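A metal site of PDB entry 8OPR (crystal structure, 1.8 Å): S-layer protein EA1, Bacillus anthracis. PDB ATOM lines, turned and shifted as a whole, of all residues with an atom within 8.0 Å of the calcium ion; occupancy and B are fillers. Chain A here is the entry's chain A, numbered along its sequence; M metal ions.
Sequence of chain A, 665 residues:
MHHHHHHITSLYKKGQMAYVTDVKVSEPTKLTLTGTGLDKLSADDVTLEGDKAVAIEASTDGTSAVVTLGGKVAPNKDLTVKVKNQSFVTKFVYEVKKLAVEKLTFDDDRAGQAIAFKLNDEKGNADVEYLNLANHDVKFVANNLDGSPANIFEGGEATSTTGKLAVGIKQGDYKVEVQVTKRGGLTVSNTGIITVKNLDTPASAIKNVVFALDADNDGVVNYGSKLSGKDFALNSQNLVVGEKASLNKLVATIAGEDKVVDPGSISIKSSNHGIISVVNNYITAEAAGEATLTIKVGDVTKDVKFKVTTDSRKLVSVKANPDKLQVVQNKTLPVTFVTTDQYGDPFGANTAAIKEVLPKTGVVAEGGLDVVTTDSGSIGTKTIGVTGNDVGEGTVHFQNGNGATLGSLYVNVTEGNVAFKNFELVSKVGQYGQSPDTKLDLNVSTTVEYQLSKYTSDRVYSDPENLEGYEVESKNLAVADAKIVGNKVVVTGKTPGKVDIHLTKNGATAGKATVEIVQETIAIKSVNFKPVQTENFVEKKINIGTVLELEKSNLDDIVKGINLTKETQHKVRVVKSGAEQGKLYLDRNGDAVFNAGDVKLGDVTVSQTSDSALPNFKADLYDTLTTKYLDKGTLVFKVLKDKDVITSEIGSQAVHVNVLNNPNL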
ATOM      1  N   ASP A 556      16.708  -1.342   3.522  1.00  0.00           N
ATOM      2  CA  ASP A 556      16.833  -1.578   2.080  1.00  0.00           C
ATOM      3  C   ASP A 556      17.965  -0.707   1.486  1.00  0.00           C
ATOM      4  O   ASP A 556      18.003   0.483   1.748  1.00  0.00           O
ATOM      5  CB  ASP A 556      15.493  -1.282   1.369  1.00  0.00           C
ATOM      6  CG  ASP A 556      14.380  -2.255   1.706  1.00  0.00           C
ATOM      7  OD1 ASP A 556      14.681  -3.338   2.259  1.00  0.00           O
ATOM      8  OD2 ASP A 556      13.202  -1.950   1.398  1.00  0.00           O
ATOM      9  N   ARG A 573      15.692   2.316  -4.188  1.00  0.00           N
ATOM     10  CA  ARG A 573      16.097   1.266  -3.286  1.00  0.00           C
ATOM     11  C   ARG A 573      15.633  -0.080  -3.807  1.00  0.00           C
ATOM     12  O   ARG A 573      14.878  -0.144  -4.774  1.00  0.00           O
ATOM     13  CB  ARG A 573      15.580   1.523  -1.864  1.00  0.00           C
ATOM     14  CG  ARG A 573      16.106   2.793  -1.254  1.00  0.00           C
ATOM     15  CD  ARG A 573      15.831   2.852   0.232  1.00  0.00           C
ATOM     16  NE  ARG A 573      16.286   4.119   0.798  1.00  0.00           N
ATOM     17  CZ  ARG A 573      17.408   4.280   1.495  1.00  0.00           C
ATOM     18  NH1 ARG A 573      18.194   3.227   1.743  1.00  0.00           N
ATOM     19  NH2 ARG A 573      17.755   5.473   1.945  1.00  0.00           N
ATOM     20  N   TYR A 585      12.182   0.316  -5.946  1.00  0.00           N
ATOM     21  CA  TYR A 585      11.192   1.336  -5.672  1.00  0.00           C
ATOM     22  C   TYR A 585      11.804   2.698  -5.443  1.00  0.00           C
ATOM     23  O   TYR A 585      12.949   2.808  -4.990  1.00  0.00           O
ATOM     24  CB  TYR A 585      10.291   0.927  -4.494  1.00  0.00           C
ATOM     25  CG  TYR A 585      11.027   0.869  -3.157  1.00  0.00           C
ATOM     26  CD1 TYR A 585      11.020   1.947  -2.299  1.00  0.00           C
ATOM     27  CD2 TYR A 585      11.618  -0.308  -2.721  1.00  0.00           C
ATOM     28  CE1 TYR A 585      11.670   1.905  -1.066  1.00  0.00           C
ATOM     29  CE2 TYR A 585      12.270  -0.373  -1.489  1.00  0.00           C
ATOM     30  CZ  TYR A 585      12.281   0.744  -0.666  1.00  0.00           C
ATOM     31  OH  TYR A 585      12.929   0.712   0.539  1.00  0.00           O
ATOM     32  N   LEU A 586      11.029   3.736  -5.726  1.00  0.00           N
ATOM     33  CA  LEU A 586      11.461   5.098  -5.451  1.00  0.00           C
ATOM     34  C   LEU A 586      11.009   5.381  -4.008  1.00  0.00           C
ATOM     35  O   LEU A 586       9.825   5.329  -3.699  1.00  0.00           O
ATOM     36  CB  LEU A 586      10.833   6.097  -6.435  1.00  0.00           C
ATOM     37  CG  LEU A 586      11.423   7.511  -6.316  1.00  0.00           C
ATOM     38  CD1 LEU A 586      12.839   7.539  -6.769  1.00  0.00           C
ATOM     39  CD2 LEU A 586      10.599   8.508  -7.134  1.00  0.00           C
ATOM     40  N   ASP A 587      11.960   5.600  -3.129  1.00  0.00           N
ATOM     41  CA  ASP A 587      11.700   5.820  -1.723  1.00  0.00           C
ATOM     42  C   ASP A 587      11.335   7.299  -1.492  1.00  0.00           C
ATOM     43  O   ASP A 587      12.188   8.117  -1.167  1.00  0.00           O
ATOM     44  CB  ASP A 587      12.918   5.374  -0.926  1.00  0.00           C
ATOM     45  CG  ASP A 587      12.686   5.284   0.550  1.00  0.00           C
ATOM     46  OD1 ASP A 587      11.508   5.143   0.958  1.00  0.00           O
ATOM     47  OD2 ASP A 587      13.653   5.366   1.290  1.00  0.00           O
ATOM     48  N   ARG A 588      10.067   7.617  -1.709  1.00  0.00           N
ATOM     49  CA  ARG A 588       9.554   8.972  -1.664  1.00  0.00           C
ATOM     50  C   ARG A 588       9.534   9.620  -0.260  1.00  0.00           C
ATOM     51  O   ARG A 588       9.598  10.845  -0.166  1.00  0.00           O
ATOM     52  CB  ARG A 588       8.185   9.055  -2.344  1.00  0.00           C
ATOM     53  CG  ARG A 588       8.267   8.764  -3.844  1.00  0.00           C
ATOM     54  CD  ARG A 588       7.010   9.153  -4.604  1.00  0.00           C
ATOM     55  NE  ARG A 588       6.696  10.570  -4.432  1.00  0.00           N
ATOM     56  CZ  ARG A 588       5.691  11.028  -3.691  1.00  0.00           C
ATOM     57  NH1 ARG A 588       4.873  10.189  -3.069  1.00  0.00           N
ATOM     58  NH2 ARG A 588       5.476  12.333  -3.585  1.00  0.00           N
ATOM     59  N   ASN A 589       9.499   8.818   0.812  1.00  0.00           N
ATOM     60  CA  ASN A 589       9.571   9.353   2.171  1.00  0.00           C
ATOM     61  C   ASN A 589      10.974   9.211   2.820  1.00  0.00           C
ATOM     62  O   ASN A 589      11.215   9.791   3.881  1.00  0.00           O
ATOM     63  CB  ASN A 589       8.467   8.807   3.072  1.00  0.00           C
ATOM     64  CG  ASN A 589       8.364   7.316   3.086  1.00  0.00           C
ATOM     65  OD1 ASN A 589       9.156   6.601   2.474  1.00  0.00           O
ATOM     66  ND2 ASN A 589       7.360   6.816   3.781  1.00  0.00           N
ATOM     67  N   GLY A 590      11.892   8.493   2.170  1.00  0.00           N
ATOM     68  CA  GLY A 590      13.280   8.382   2.583  1.00  0.00           C
ATOM     69  C   GLY A 590      13.579   7.532   3.807  1.00  0.00           C
ATOM     70  O   GLY A 590      14.634   7.693   4.413  1.00  0.00           O
ATOM     71  N   ASP A 591      12.694   6.597   4.142  1.00  0.00           N
ATOM     72  CA  ASP A 591      12.865   5.776   5.335  1.00  0.00           C
ATOM     73  C   ASP A 591      13.483   4.362   5.121  1.00  0.00           C
ATOM     74  O   ASP A 591      13.486   3.568   6.065  1.00  0.00           O
ATOM     75  CB  ASP A 591      11.519   5.644   6.063  1.00  0.00           C
ATOM     76  CG  ASP A 591      10.411   4.980   5.267  1.00  0.00           C
ATOM     77  OD1 ASP A 591      10.643   4.670   4.076  1.00  0.00           O
ATOM     78  OD2 ASP A 591       9.318   4.777   5.822  1.00  0.00           O
ATOM     79  N   ALA A 592      13.976   4.061   3.895  1.00  0.00           N
ATOM     80  CA  ALA A 592      14.616   2.789   3.509  1.00  0.00           C
ATOM     81  C   ALA A 592      13.735   1.564   3.703  1.00  0.00           C
ATOM     82  O   ALA A 592      14.243   0.475   3.947  1.00  0.00           O
ATOM     83  CB  ALA A 592      15.952   2.601   4.215  1.00  0.00           C
ATOM     84  N   VAL A 593      12.416   1.740   3.580  1.00  0.00           N
ATOM     85  CA  VAL A 593      11.405   0.684   3.690  1.00  0.00           C
ATOM     86  C   VAL A 593      10.352   0.954   2.614  1.00  0.00           C
ATOM     87  O   VAL A 593      10.011   2.107   2.394  1.00  0.00           O
ATOM     88  CB  VAL A 593      10.759   0.623   5.112  1.00  0.00           C
ATOM     89  CG1 VAL A 593       9.487  -0.230   5.116  1.00  0.00           C
ATOM     90  CG2 VAL A 593      11.741   0.093   6.157  1.00  0.00           C
ATOM     91  N   PHE A 594       9.874  -0.089   1.905  1.00  0.00           N
ATOM     92  CA  PHE A 594       8.850   0.105   0.885  1.00  0.00           C
ATOM     93  C   PHE A 594       7.493   0.247   1.565  1.00  0.00           C
ATOM     94  O   PHE A 594       7.019  -0.697   2.207  1.00  0.00           O
ATOM     95  CB  PHE A 594       8.816  -1.041  -0.139  1.00  0.00           C
ATOM     96  CG  PHE A 594       7.733  -0.869  -1.169  1.00  0.00           C
ATOM     97  CD1 PHE A 594       7.748   0.193  -2.046  1.00  0.00           C
ATOM     98  CD2 PHE A 594       6.653  -1.735  -1.212  1.00  0.00           C
ATOM     99  CE1 PHE A 594       6.745   0.363  -2.992  1.00  0.00           C
ATOM    100  CE2 PHE A 594       5.632  -1.553  -2.135  1.00  0.00           C
ATOM    101  CZ  PHE A 594       5.693  -0.510  -3.023  1.00  0.00           C
ATOM    102  N   ASN A 595       6.853   1.405   1.407  1.00  0.00           N
ATOM    103  CA  ASN A 595       5.585   1.679   2.079  1.00  0.00           C
ATOM    104  C   ASN A 595       4.870   2.904   1.456  1.00  0.00           C
ATOM    105  O   ASN A 595       5.107   3.221   0.278  1.00  0.00           O
ATOM    106  CB  ASN A 595       5.874   1.889   3.608  1.00  0.00           C
ATOM    107  CG  ASN A 595       6.899   2.956   3.909  1.00  0.00           C
ATOM    108  OD1 ASN A 595       7.210   3.824   3.089  1.00  0.00           O
ATOM    109  ND2 ASN A 595       7.455   2.927   5.106  1.00  0.00           N
ATOM    110  N   ALA A 596       3.942   3.532   2.224  1.00  0.00           N
ATOM    111  CA  ALA A 596       3.222   4.780   2.034  1.00  0.00           C
ATOM    112  C   ALA A 596       3.117   5.223   0.508  1.00  0.00           C
ATOM    113  O   ALA A 596       2.436   4.499  -0.204  1.00  0.00           O
ATOM    114  CB  ALA A 596       3.840   5.855   2.968  1.00  0.00           C
ATOM    115  N   GLY A 597       3.718   6.317   0.010  1.00  0.00           N
ATOM    116  CA  GLY A 597       3.574   6.725  -1.376  1.00  0.00           C
ATOM    117  C   GLY A 597       4.804   6.442  -2.204  1.00  0.00           C
ATOM    118  O   GLY A 597       5.164   7.243  -3.070  1.00  0.00           O
ATOM    119  N   ASP A 598       5.494   5.331  -1.904  1.00  0.00           N
ATOM    120  CA  ASP A 598       6.662   4.924  -2.673  1.00  0.00           C
ATOM    121  C   ASP A 598       6.163   4.370  -3.999  1.00  0.00           C
ATOM    122  O   ASP A 598       5.065   3.800  -4.068  1.00  0.00           O
ATOM    123  CB  ASP A 598       7.464   3.826  -1.942  1.00  0.00           C
ATOM    124  CG  ASP A 598       8.164   4.293  -0.684  1.00  0.00           C
ATOM    125  OD1 ASP A 598       8.373   5.534  -0.551  1.00  0.00           O
ATOM    126  OD2 ASP A 598       8.504   3.439   0.155  1.00  0.00           O
ATOM    127  N   VAL A 599       6.946   4.547  -5.052  1.00  0.00           N
ATOM    128  CA  VAL A 599       6.560   4.058  -6.383  1.00  0.00           C
ATOM    129  C   VAL A 599       7.317   2.805  -6.706  1.00  0.00           C
ATOM    130  O   VAL A 599       8.523   2.866  -6.737  1.00  0.00           O
ATOM    131  CB  VAL A 599       6.872   5.125  -7.453  1.00  0.00           C
ATOM    132  CG1 VAL A 599       6.419   4.661  -8.840  1.00  0.00           C
ATOM    133  CG2 VAL A 599       6.264   6.475  -7.082  1.00  0.00           C
HETATM  134 CA    CA M   1       9.614   4.254   2.015  1.00  0.00          CA
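The side-chain hydroxyl of Tyr 585 is in hydrogen-bond range of the backbone NH of Val 593, at 3.3 Å.
The backbone NH (N) of Arg 588 lies within hydrogen-bond range of the side-chain carboxylate (OD1) of Asp 598.
The backbone NH of Ala 592 lies within hydrogen-bond range of the side-chain carboxylate of Asp 587 (2.9 Å).
OD2 of Asp 587 is in salt-bridge range of NE of Arg 573.
Within 4 Å of the calcium ion: Asp 587, Asn 589, Asp 591, Val 593, Asn 595 and Asp 598.
Along chain A the residues within 4 Å of the calcium ion span positions 587 to 598.
The nearest printed residue that does not touch the calcium ion is Phe 594 (4.4 Å).
The calcium ion is bound by O of Val 593 (2.2 Å), OD2 of Asp 598 (2.3 Å), OD1 of Asp 591 (2.3 Å), OD1 of Asp 587 (2.3 Å), OD1 of Asn 589 (2.4 Å) and OD1 of Asn 595 (2.7 Å).
Slightly farther from the calcium ion lies the side-chain carboxylate (OD1) of Asp 598 (3.1 Å).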
